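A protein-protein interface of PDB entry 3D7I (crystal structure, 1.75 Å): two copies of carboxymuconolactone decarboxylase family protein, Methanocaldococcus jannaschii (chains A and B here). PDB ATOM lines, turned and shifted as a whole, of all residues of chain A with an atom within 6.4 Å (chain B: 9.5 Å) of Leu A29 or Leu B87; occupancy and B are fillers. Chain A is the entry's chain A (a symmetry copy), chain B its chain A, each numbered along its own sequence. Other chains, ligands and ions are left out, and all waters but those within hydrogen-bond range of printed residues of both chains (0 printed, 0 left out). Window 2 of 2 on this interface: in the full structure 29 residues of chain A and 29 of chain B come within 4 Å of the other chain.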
ATOM      1  N   ASP A  24      -1.567  24.938  -4.306  1.00  0.00           N
ATOM      2  CA  ASP A  24      -2.629  24.369  -3.480  1.00  0.00           C
ATOM      3  C   ASP A  24      -3.807  23.937  -4.344  1.00  0.00           C
ATOM      4  O   ASP A  24      -4.313  22.816  -4.213  1.00  0.00           O
ATOM      5  CB  ASP A  24      -3.102  25.402  -2.453  1.00  0.00           C
ATOM      6  CG  ASP A  24      -4.249  24.898  -1.596  1.00  0.00           C
ATOM      7  OD1 ASP A  24      -4.013  24.019  -0.745  1.00  0.00           O
ATOM      8  OD2 ASP A  24      -5.385  25.381  -1.767  1.00  0.00           O
ATOM      9  N   ILE A  25      -4.254  24.825  -5.229  1.00  0.00           N
ATOM     10  CA  ILE A  25      -5.399  24.462  -6.088  1.00  0.00           C
ATOM     11  C   ILE A  25      -5.048  23.351  -7.086  1.00  0.00           C
ATOM     12  O   ILE A  25      -5.890  22.459  -7.362  1.00  0.00           O
ATOM     13  CB  ILE A  25      -6.068  25.688  -6.754  1.00  0.00           C
ATOM     14  CG1 ILE A  25      -7.437  25.287  -7.333  1.00  0.00           C
ATOM     15  CG2 ILE A  25      -5.184  26.284  -7.838  1.00  0.00           C
ATOM     16  CD1 ILE A  25      -8.418  24.769  -6.300  1.00  0.00           C
ATOM     17  N   ILE A  26      -3.816  23.343  -7.592  1.00  0.00           N
ATOM     18  CA  ILE A  26      -3.359  22.276  -8.460  1.00  0.00           C
ATOM     19  C   ILE A  26      -3.420  20.903  -7.779  1.00  0.00           C
ATOM     20  O   ILE A  26      -3.909  19.923  -8.351  1.00  0.00           O
ATOM     21  CB  ILE A  26      -1.937  22.558  -8.977  1.00  0.00           C
ATOM     22  CG1 ILE A  26      -1.979  23.678 -10.053  1.00  0.00           C
ATOM     23  CG2 ILE A  26      -1.314  21.274  -9.490  1.00  0.00           C
ATOM     24  CD1 ILE A  26      -0.615  24.212 -10.426  1.00  0.00           C
ATOM     25  N   VAL A  27      -2.935  20.824  -6.549  1.00  0.00           N
ATOM     26  CA  VAL A  27      -2.998  19.575  -5.812  1.00  0.00           C
ATOM     27  C   VAL A  27      -4.453  19.150  -5.603  1.00  0.00           C
ATOM     28  O   VAL A  27      -4.799  17.974  -5.775  1.00  0.00           O
ATOM     29  CB  VAL A  27      -2.290  19.656  -4.453  1.00  0.00           C
ATOM     30  CG1 VAL A  27      -2.486  18.335  -3.687  1.00  0.00           C
ATOM     31  CG2 VAL A  27      -0.785  19.974  -4.652  1.00  0.00           C
ATOM     32  N   LYS A  28      -5.294  20.089  -5.193  1.00  0.00           N
ATOM     33  CA  LYS A  28      -6.707  19.799  -4.965  1.00  0.00           C
ATOM     34  C   LYS A  28      -7.425  19.392  -6.248  1.00  0.00           C
ATOM     35  O   LYS A  28      -8.251  18.472  -6.250  1.00  0.00           O
ATOM     36  CB  LYS A  28      -7.391  20.983  -4.276  1.00  0.00           C
ATOM     37  CG  LYS A  28      -6.810  21.192  -2.878  1.00  0.00           C
ATOM     38  CD  LYS A  28      -7.653  22.050  -1.919  1.00  0.00           C
ATOM     39  CE  LYS A  28      -7.777  23.479  -2.364  1.00  0.00           C
ATOM     40  NZ  LYS A  28      -8.135  24.322  -1.184  1.00  0.00           N
ATOM     41  N   LEU A  29      -7.106  20.065  -7.342  1.00  0.00           N
ATOM     42  CA  LEU A  29      -7.602  19.695  -8.657  1.00  0.00           C
ATOM     43  C   LEU A  29      -7.236  18.255  -8.986  1.00  0.00           C
ATOM     44  O   LEU A  29      -8.112  17.424  -9.333  1.00  0.00           O
ATOM     45  CB  LEU A  29      -7.051  20.619  -9.730  1.00  0.00           C
ATOM     46  CG  LEU A  29      -7.508  20.267 -11.170  1.00  0.00           C
ATOM     47  CD1 LEU A  29      -9.001  20.544 -11.323  1.00  0.00           C
ATOM     48  CD2 LEU A  29      -6.619  21.028 -12.180  1.00  0.00           C
ATOM     49  N   ASN A  30      -5.958  17.936  -8.848  1.00  0.00           N
ATOM     50  CA  ASN A  30      -5.512  16.583  -9.097  1.00  0.00           C
ATOM     51  C   ASN A  30      -6.285  15.562  -8.244  1.00  0.00           C
ATOM     52  O   ASN A  30      -6.740  14.530  -8.755  1.00  0.00           O
ATOM     53  CB  ASN A  30      -4.002  16.499  -8.836  1.00  0.00           C
ATOM     54  CG  ASN A  30      -3.451  15.140  -9.109  1.00  0.00           C
ATOM     55  OD1 ASN A  30      -3.098  14.828 -10.224  1.00  0.00           O
ATOM     56  ND2 ASN A  30      -3.350  14.337  -8.083  1.00  0.00           N
ATOM     57  N   ASP A  31      -6.407  15.842  -6.941  1.00  0.00           N
ATOM     58  CA  ASP A  31      -7.054  14.934  -6.007  1.00  0.00           C
ATOM     59  C   ASP A  31      -8.529  14.729  -6.340  1.00  0.00           C
ATOM     60  O   ASP A  31      -9.010  13.587  -6.340  1.00  0.00           O
ATOM     61  CB  ASP A  31      -6.889  15.429  -4.580  1.00  0.00           C
ATOM     62  CG  ASP A  31      -5.458  15.318  -4.090  1.00  0.00           C
ATOM     63  OD1 ASP A  31      -4.607  14.729  -4.787  1.00  0.00           O
ATOM     64  OD2 ASP A  31      -5.185  15.926  -3.053  1.00  0.00           O
ATOM     65  N   THR A  32      -9.213  15.804  -6.718  1.00  0.00           N
ATOM     66  CA  THR A  32     -10.629  15.743  -7.055  1.00  0.00           C
ATOM     67  C   THR A  32     -10.863  15.080  -8.390  1.00  0.00           C
ATOM     68  O   THR A  32     -11.796  14.280  -8.544  1.00  0.00           O
ATOM     69  CB  THR A  32     -11.267  17.152  -7.014  1.00  0.00           C
ATOM     70  OG1 THR A  32     -11.067  17.694  -5.683  1.00  0.00           O
ATOM     71  CG2 THR A  32     -12.757  17.110  -7.346  1.00  0.00           C
ATOM     72  N   VAL A  33     -10.014  15.382  -9.375  1.00  0.00           N
ATOM     73  CA  VAL A  33     -10.119  14.737 -10.690  1.00  0.00           C
ATOM     74  C   VAL A  33     -10.032  13.237 -10.544  1.00  0.00           C
ATOM     75  O   VAL A  33     -10.840  12.492 -11.128  1.00  0.00           O
ATOM     76  CB  VAL A  33      -9.012  15.247 -11.637  1.00  0.00           C
ATOM     77  CG1 VAL A  33      -8.687  14.239 -12.775  1.00  0.00           C
ATOM     78  CG2 VAL A  33      -9.399  16.647 -12.238  1.00  0.00           C
ATOM     79  N   PHE A  34      -9.076  12.783  -9.724  1.00  0.00           N
ATOM     80  CA  PHE A  34      -8.838  11.356  -9.530  1.00  0.00           C
ATOM     81  C   PHE A  34      -9.649  10.696  -8.396  1.00  0.00           C
ATOM     82  O   PHE A  34      -9.323   9.588  -7.957  1.00  0.00           O
ATOM     83  CB  PHE A  34      -7.327  11.092  -9.413  1.00  0.00           C
ATOM     84  CG  PHE A  34      -6.587  11.260 -10.704  1.00  0.00           C
ATOM     85  CD1 PHE A  34      -6.892  10.464 -11.800  1.00  0.00           C
ATOM     86  CD2 PHE A  34      -5.554  12.183 -10.826  1.00  0.00           C
ATOM     87  CE1 PHE A  34      -6.219  10.620 -13.028  1.00  0.00           C
ATOM     88  CE2 PHE A  34      -4.853  12.317 -12.023  1.00  0.00           C
ATOM     89  CZ  PHE A  34      -5.168  11.543 -13.115  1.00  0.00           C
ATOM     90  N   GLY B  50     -11.891   9.808 -23.820  1.00  0.00           N
ATOM     91  CA  GLY B  50     -11.004  10.777 -23.249  1.00  0.00           C
ATOM     92  C   GLY B  50     -10.165  11.453 -24.304  1.00  0.00           C
ATOM     93  O   GLY B  50      -9.978  12.680 -24.336  1.00  0.00           O
ATOM     94  N   ALA B  53     -12.424  13.638 -26.610  1.00  0.00           N
ATOM     95  CA  ALA B  53     -12.897  14.782 -25.802  1.00  0.00           C
ATOM     96  C   ALA B  53     -11.810  15.813 -25.556  1.00  0.00           C
ATOM     97  O   ALA B  53     -12.109  16.979 -25.321  1.00  0.00           O
ATOM     98  CB  ALA B  53     -13.532  14.318 -24.482  1.00  0.00           C
ATOM     99  N   SER B  54     -10.538  15.417 -25.626  1.00  0.00           N
ATOM    100  CA  SER B  54      -9.449  16.342 -25.414  1.00  0.00           C
ATOM    101  C   SER B  54      -9.210  17.250 -26.607  1.00  0.00           C
ATOM    102  O   SER B  54      -8.449  18.212 -26.485  1.00  0.00           O
ATOM    103  CB  SER B  54      -8.156  15.596 -25.051  1.00  0.00           C
ATOM    104  OG  SER B  54      -7.588  14.945 -26.171  1.00  0.00           O
ATOM    105  N   ILE B  79     -18.893   8.658 -17.916  1.00  0.00           N
ATOM    106  CA  ILE B  79     -18.285   9.522 -18.900  1.00  0.00           C
ATOM    107  C   ILE B  79     -17.750  10.783 -18.225  1.00  0.00           C
ATOM    108  O   ILE B  79     -16.656  11.273 -18.547  1.00  0.00           O
ATOM    109  CB  ILE B  79     -19.251   9.862 -20.048  1.00  0.00           C
ATOM    110  CG1 ILE B  79     -19.613   8.565 -20.790  1.00  0.00           C
ATOM    111  CG2 ILE B  79     -18.576  10.855 -21.002  1.00  0.00           C
ATOM    112  CD1 ILE B  79     -20.690   8.694 -21.853  1.00  0.00           C
ATOM    113  N   ALA B  80     -18.499  11.333 -17.280  1.00  0.00           N
ATOM    114  CA  ALA B  80     -18.021  12.495 -16.543  1.00  0.00           C
ATOM    115  C   ALA B  80     -16.684  12.228 -15.806  1.00  0.00           C
ATOM    116  O   ALA B  80     -15.854  13.127 -15.713  1.00  0.00           O
ATOM    117  CB  ALA B  80     -19.133  13.003 -15.573  1.00  0.00           C
ATOM    118  N   ASP B  81     -16.487  11.012 -15.300  1.00  0.00           N
ATOM    119  CA  ASP B  81     -15.222  10.611 -14.674  1.00  0.00           C
ATOM    120  C   ASP B  81     -14.089  10.659 -15.684  1.00  0.00           C
ATOM    121  O   ASP B  81     -12.960  10.994 -15.335  1.00  0.00           O
ATOM    122  CB  ASP B  81     -15.293   9.217 -14.060  1.00  0.00           C
ATOM    123  CG  ASP B  81     -16.086   9.157 -12.750  1.00  0.00           C
ATOM    124  OD1 ASP B  81     -16.380  10.220 -12.168  1.00  0.00           O
ATOM    125  OD2 ASP B  81     -16.398   8.024 -12.341  1.00  0.00           O
ATOM    126  N   VAL B  82     -14.375  10.316 -16.942  1.00  0.00           N
ATOM    127  CA  VAL B  82     -13.418  10.504 -18.026  1.00  0.00           C
ATOM    128  C   VAL B  82     -13.101  11.979 -18.231  1.00  0.00           C
ATOM    129  O   VAL B  82     -11.944  12.367 -18.333  1.00  0.00           O
ATOM    130  CB  VAL B  82     -13.908   9.879 -19.361  1.00  0.00           C
ATOM    131  CG1 VAL B  82     -12.902  10.109 -20.510  1.00  0.00           C
ATOM    132  CG2 VAL B  82     -14.216   8.326 -19.208  1.00  0.00           C
ATOM    133  N   LEU B  83     -14.148  12.791 -18.256  1.00  0.00           N
ATOM    134  CA  LEU B  83     -14.006  14.227 -18.463  1.00  0.00           C
ATOM    135  C   LEU B  83     -13.230  14.934 -17.359  1.00  0.00           C
ATOM    136  O   LEU B  83     -12.530  15.901 -17.619  1.00  0.00           O
ATOM    137  CB  LEU B  83     -15.368  14.860 -18.720  1.00  0.00           C
ATOM    138  CG  LEU B  83     -16.136  14.334 -19.928  1.00  0.00           C
ATOM    139  CD1 LEU B  83     -17.399  15.232 -20.182  1.00  0.00           C
ATOM    140  CD2 LEU B  83     -15.256  14.229 -21.207  1.00  0.00           C
ATOM    141  N   ARG B  84     -13.267  14.393 -16.137  1.00  0.00           N
ATOM    142  CA  ARG B  84     -12.384  14.890 -15.071  1.00  0.00           C
ATOM    143  C   ARG B  84     -10.926  14.851 -15.518  1.00  0.00           C
ATOM    144  O   ARG B  84     -10.183  15.808 -15.379  1.00  0.00           O
ATOM    145  CB  ARG B  84     -12.586  14.083 -13.793  1.00  0.00           C
ATOM    146  CG  ARG B  84     -13.884  14.286 -13.093  1.00  0.00           C
ATOM    147  CD  ARG B  84     -13.928  13.446 -11.806  1.00  0.00           C
ATOM    148  NE  ARG B  84     -15.257  13.557 -11.266  1.00  0.00           N
ATOM    149  CZ  ARG B  84     -15.618  14.159 -10.140  1.00  0.00           C
ATOM    150  NH1 ARG B  84     -14.731  14.577  -9.207  1.00  0.00           N
ATOM    151  NH2 ARG B  84     -16.904  14.184  -9.865  1.00  0.00           N
ATOM    152  N   VAL B  85     -10.521  13.738 -16.116  1.00  0.00           N
ATOM    153  CA  VAL B  85      -9.166  13.566 -16.635  1.00  0.00           C
ATOM    154  C   VAL B  85      -8.893  14.503 -17.784  1.00  0.00           C
ATOM    155  O   VAL B  85      -7.801  15.067 -17.905  1.00  0.00           O
ATOM    156  CB  VAL B  85      -8.911  12.092 -17.010  1.00  0.00           C
ATOM    157  CG1 VAL B  85      -7.431  11.906 -17.396  1.00  0.00           C
ATOM    158  CG2 VAL B  85      -9.265  11.141 -15.820  1.00  0.00           C
ATOM    159  N   VAL B  86      -9.899  14.724 -18.639  1.00  0.00           N
ATOM    160  CA  VAL B  86      -9.755  15.680 -19.760  1.00  0.00           C
ATOM    161  C   VAL B  86      -9.420  17.083 -19.237  1.00  0.00           C
ATOM    162  O   VAL B  86      -8.506  17.737 -19.738  1.00  0.00           O
ATOM    163  CB  VAL B  86     -11.035  15.701 -20.616  1.00  0.00           C
ATOM    164  CG1 VAL B  86     -10.964  16.810 -21.667  1.00  0.00           C
ATOM    165  CG2 VAL B  86     -11.228  14.260 -21.299  1.00  0.00           C
ATOM    166  N   LEU B  87     -10.127  17.506 -18.192  1.00  0.00           N
ATOM    167  CA  LEU B  87      -9.883  18.812 -17.567  1.00  0.00           C
ATOM    168  C   LEU B  87      -8.433  18.918 -17.129  1.00  0.00           C
ATOM    169  O   LEU B  87      -7.738  19.882 -17.450  1.00  0.00           O
ATOM    170  CB  LEU B  87     -10.803  19.006 -16.378  1.00  0.00           C
ATOM    171  CG  LEU B  87     -10.540  20.251 -15.495  1.00  0.00           C
ATOM    172  CD1 LEU B  87     -10.631  21.524 -16.337  1.00  0.00           C
ATOM    173  CD2 LEU B  87     -11.473  20.225 -14.253  1.00  0.00           C
ATOM    174  N   LEU B  88      -7.960  17.923 -16.389  1.00  0.00           N
ATOM    175  CA  LEU B  88      -6.601  17.998 -15.830  1.00  0.00           C
ATOM    176  C   LEU B  88      -5.539  18.029 -16.920  1.00  0.00           C
ATOM    177  O   LEU B  88      -4.541  18.778 -16.857  1.00  0.00           O
ATOM    178  CB  LEU B  88      -6.382  16.830 -14.893  1.00  0.00           C
ATOM    179  CG  LEU B  88      -5.042  16.782 -14.143  1.00  0.00           C
ATOM    180  CD1 LEU B  88      -4.989  17.873 -13.091  1.00  0.00           C
ATOM    181  CD2 LEU B  88      -4.872  15.439 -13.483  1.00  0.00           C
ATOM    182  N   THR B  89      -5.740  17.199 -17.947  1.00  0.00           N
ATOM    183  CA  THR B  89      -4.743  17.004 -18.995  1.00  0.00           C
ATOM    184  C   THR B  89      -4.840  18.026 -20.101  1.00  0.00           C
ATOM    185  O   THR B  89      -3.894  18.236 -20.852  1.00  0.00           O
ATOM    186  CB  THR B  89      -4.867  15.614 -19.665  1.00  0.00           C
ATOM    187  OG1 THR B  89      -6.194  15.473 -20.218  1.00  0.00           O
ATOM    188  CG2 THR B  89      -4.582  14.468 -18.662  1.00  0.00           C
ATOM    189  N   SER B  90      -5.998  18.645 -20.233  1.00  0.00           N
ATOM    190  CA  SER B  90      -6.315  19.397 -21.448  1.00  0.00           C
ATOM    191  C   SER B  90      -6.951  20.766 -21.275  1.00  0.00           C
ATOM    192  O   SER B  90      -7.022  21.531 -22.240  1.00  0.00           O
ATOM    193  CB  SER B  90      -7.195  18.535 -22.372  1.00  0.00           C
ATOM    194  OG  SER B  90      -6.661  17.234 -22.569  1.00  0.00           O
ATOM    195  N   GLY B  91      -7.416  21.082 -20.075  1.00  0.00           N
ATOM    196  CA  GLY B  91      -7.917  22.417 -19.787  1.00  0.00           C
ATOM    197  C   GLY B  91      -9.428  22.576 -19.823  1.00  0.00           C
ATOM    198  O   GLY B  91     -10.165  21.649 -20.230  1.00  0.00           O
ATOM    199  N   MET B  92      -9.868  23.760 -19.416  1.00  0.00           N
ATOM    200  CA  MET B  92     -11.291  24.109 -19.302  1.00  0.00           C
ATOM    201  C   MET B  92     -12.060  24.110 -20.624  1.00  0.00           C
ATOM    202  O   MET B  92     -13.172  23.597 -20.664  1.00  0.00           O
ATOM    203  CB  MET B  92     -11.490  25.438 -18.552  1.00  0.00           C
ATOM    204  CG  MET B  92     -11.341  25.286 -17.130  1.00  0.00           C
ATOM    205  SD  MET B  92     -12.922  24.433 -16.419  1.00  0.00           S
ATOM    206  CE  MET B  92     -14.193  25.863 -16.692  1.00  0.00           C
ATOM    207  N   PRO B  93     -11.498  24.673 -21.713  1.00  0.00           N
ATOM    208  CA  PRO B  93     -12.303  24.645 -22.953  1.00  0.00           C
ATOM    209  C   PRO B  93     -12.741  23.239 -23.363  1.00  0.00           C
ATOM    210  O   PRO B  93     -13.912  23.038 -23.740  1.00  0.00           O
ATOM    211  CB  PRO B  93     -11.358  25.257 -23.988  1.00  0.00           C
ATOM    212  CG  PRO B  93     -10.557  26.241 -23.167  1.00  0.00           C
ATOM    213  CD  PRO B  93     -10.251  25.430 -21.911  1.00  0.00           C
ATOM    214  N   ALA B  94     -11.815  22.282 -23.324  1.00  0.00           N
ATOM    215  CA  ALA B  94     -12.121  20.903 -23.707  1.00  0.00           C
ATOM    216  C   ALA B  94     -13.098  20.310 -22.734  1.00  0.00           C
ATOM    217  O   ALA B  94     -14.079  19.658 -23.130  1.00  0.00           O
ATOM    218  CB  ALA B  94     -10.835  20.029 -23.802  1.00  0.00           C
ATOM    219  N   PHE B  95     -12.870  20.542 -21.441  1.00  0.00           N
ATOM    220  CA  PHE B  95     -13.768  20.009 -20.429  1.00  0.00           C
ATOM    221  C   PHE B  95     -15.202  20.522 -20.607  1.00  0.00           C
ATOM    222  O   PHE B  95     -16.153  19.739 -20.596  1.00  0.00           O
ATOM    223  CB  PHE B  95     -13.251  20.354 -19.035  1.00  0.00           C
ATOM    224  CG  PHE B  95     -14.207  19.972 -17.923  1.00  0.00           C
ATOM    225  CD1 PHE B  95     -14.338  18.672 -17.548  1.00  0.00           C
ATOM    226  CD2 PHE B  95     -15.002  20.930 -17.273  1.00  0.00           C
ATOM    227  CE1 PHE B  95     -15.213  18.304 -16.553  1.00  0.00           C
ATOM    228  CE2 PHE B  95     -15.884  20.544 -16.257  1.00  0.00           C
ATOM    229  CZ  PHE B  95     -15.971  19.251 -15.906  1.00  0.00           C
ATOM    230  N   THR B  96     -15.349  21.826 -20.739  1.00  0.00           N
ATOM    231  CA  THR B  96     -16.680  22.430 -20.799  1.00  0.00           C
ATOM    232  C   THR B  96     -17.430  22.051 -22.079  1.00  0.00           C
ATOM    233  O   THR B  96     -18.648  21.794 -22.030  1.00  0.00           O
ATOM    234  CB  THR B  96     -16.666  23.963 -20.567  1.00  0.00           C
ATOM    235  OG1 THR B  96     -15.897  24.605 -21.572  1.00  0.00           O
ATOM    236  CG2 THR B  96     -16.122  24.315 -19.200  1.00  0.00           C
ATOM    237  N   LYS B  97     -16.724  21.987 -23.222  1.00  0.00           N
ATOM    238  CA  LYS B  97     -17.345  21.556 -24.482  1.00  0.00           C
ATOM    239  C   LYS B  97     -17.878  20.133 -24.329  1.00  0.00           C
ATOM    240  O   LYS B  97     -19.014  19.832 -24.704  1.00  0.00           O
ATOM    241  CB  LYS B  97     -16.335  21.605 -25.634  1.00  0.00           C
ATOM    242  CG  LYS B  97     -16.833  21.065 -26.971  1.00  0.00           C
ATOM    243  CD  LYS B  97     -15.744  21.148 -28.043  1.00  0.00           C
ATOM    244  CE  LYS B  97     -16.294  20.917 -29.449  1.00  0.00           C
ATOM    245  NZ  LYS B  97     -17.028  22.123 -29.889  1.00  0.00           N
ATOM    246  N   ALA B  98     -17.039  19.260 -23.785  1.00  0.00           N
ATOM    247  CA  ALA B  98     -17.372  17.852 -23.707  1.00  0.00           C
ATOM    248  C   ALA B  98     -18.463  17.619 -22.679  1.00  0.00           C
ATOM    249  O   ALA B  98     -19.324  16.755 -22.874  1.00  0.00           O
ATOM    250  CB  ALA B  98     -16.135  17.030 -23.386  1.00  0.00           C
ATOM    251  N   MET B  99     -18.448  18.400 -21.588  1.00  0.00           N
ATOM    252  CA  MET B  99     -19.478  18.251 -20.566  1.00  0.00           C
ATOM    253  C   MET B  99     -20.847  18.709 -21.121  1.00  0.00           C
ATOM    254  O   MET B  99     -21.857  18.074 -20.856  1.00  0.00           O
ATOM    255  CB  MET B  99     -19.052  18.974 -19.276  1.00  0.00           C
ATOM    256  CG  MET B  99     -20.003  18.892 -18.126  1.00  0.00           C
ATOM    257  SD  MET B  99     -20.237  17.095 -17.476  1.00  0.00           S
ATOM    258  CE  MET B  99     -18.500  16.794 -16.652  1.00  0.00           C
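O of Thr A32 lies within hydrogen-bond range of NH1 of Arg B84, at 3.0 Å.
The backbone carbonyl oxygen of Val B85 is in hydrogen-bond range of the side-chain hydroxyl of Thr B89 (2.8 Å).
The side-chain carboxylate (OD1) of Asp B81 lies within salt-bridge range of the guanidinium group (NE) of Arg B84.
OG1 of Thr A32 sits at hydrogen-bond distance from O of Lys A28 (3.0 Å).
Among the printed residues, pairs that only touch across the chains: Leu A29 with Leu B87 (3.8 Å), Leu A29 with Leu B88 (3.7 Å), Asn A30 with Leu B88 (3.8 Å), Val A33 with Arg B84 (3.3 Å), Val A33 with Val B85 (3.8 Å) and Phe A34 with Leu B88 (3.4 Å).
Leu A29 touches two residues of chain B.
Thr A32 touches just one residue of chain B: Arg B84.
Of the printed residues of chain A, Arg B84 touches Thr A32 (3.0 Å) and Val A33 (3.3 Å).
Of the printed residues of chain A, Val B85 touches Val A33 (3.8 Å).
Of the printed residues of chain A, Leu B88 touches Leu A29 (3.7 Å), Asn A30 (3.8 Å) and Phe A34 (3.4 Å).
Of the printed residues of chain B, Phe A34 touches Leu B88 (3.4 Å).
Printed residues of chain B within 4 Å of Val A33: Arg B84 and Val B85.
Thr B96 touches none of the printed residues of chain A.
The nearest printed residue of chain B that does not touch Phe A34 is Val B85 (4.2 Å).
Of the 11 printed residues of chain A, 5 touch a printed residue of chain B.
Hydrophobic or aromatic side chains of chain A within 4 Å of the printed part of chain B: Leu A29, Val A33 and Phe A34.
Printed residues of chain B that touch a printed residue of chain A: Arg B84, Val B85, Leu B87 and Leu B88.
Hydrophobic or aromatic side chains of chain B within 4 Å of the printed part of chain A: Leu B87 and Leu B88.
Among the printed residues, no Asp or Glu carboxylate lies within 4 Å of a Lys or Arg side-chain nitrogen of the other chain.
No position is printed for both chains.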
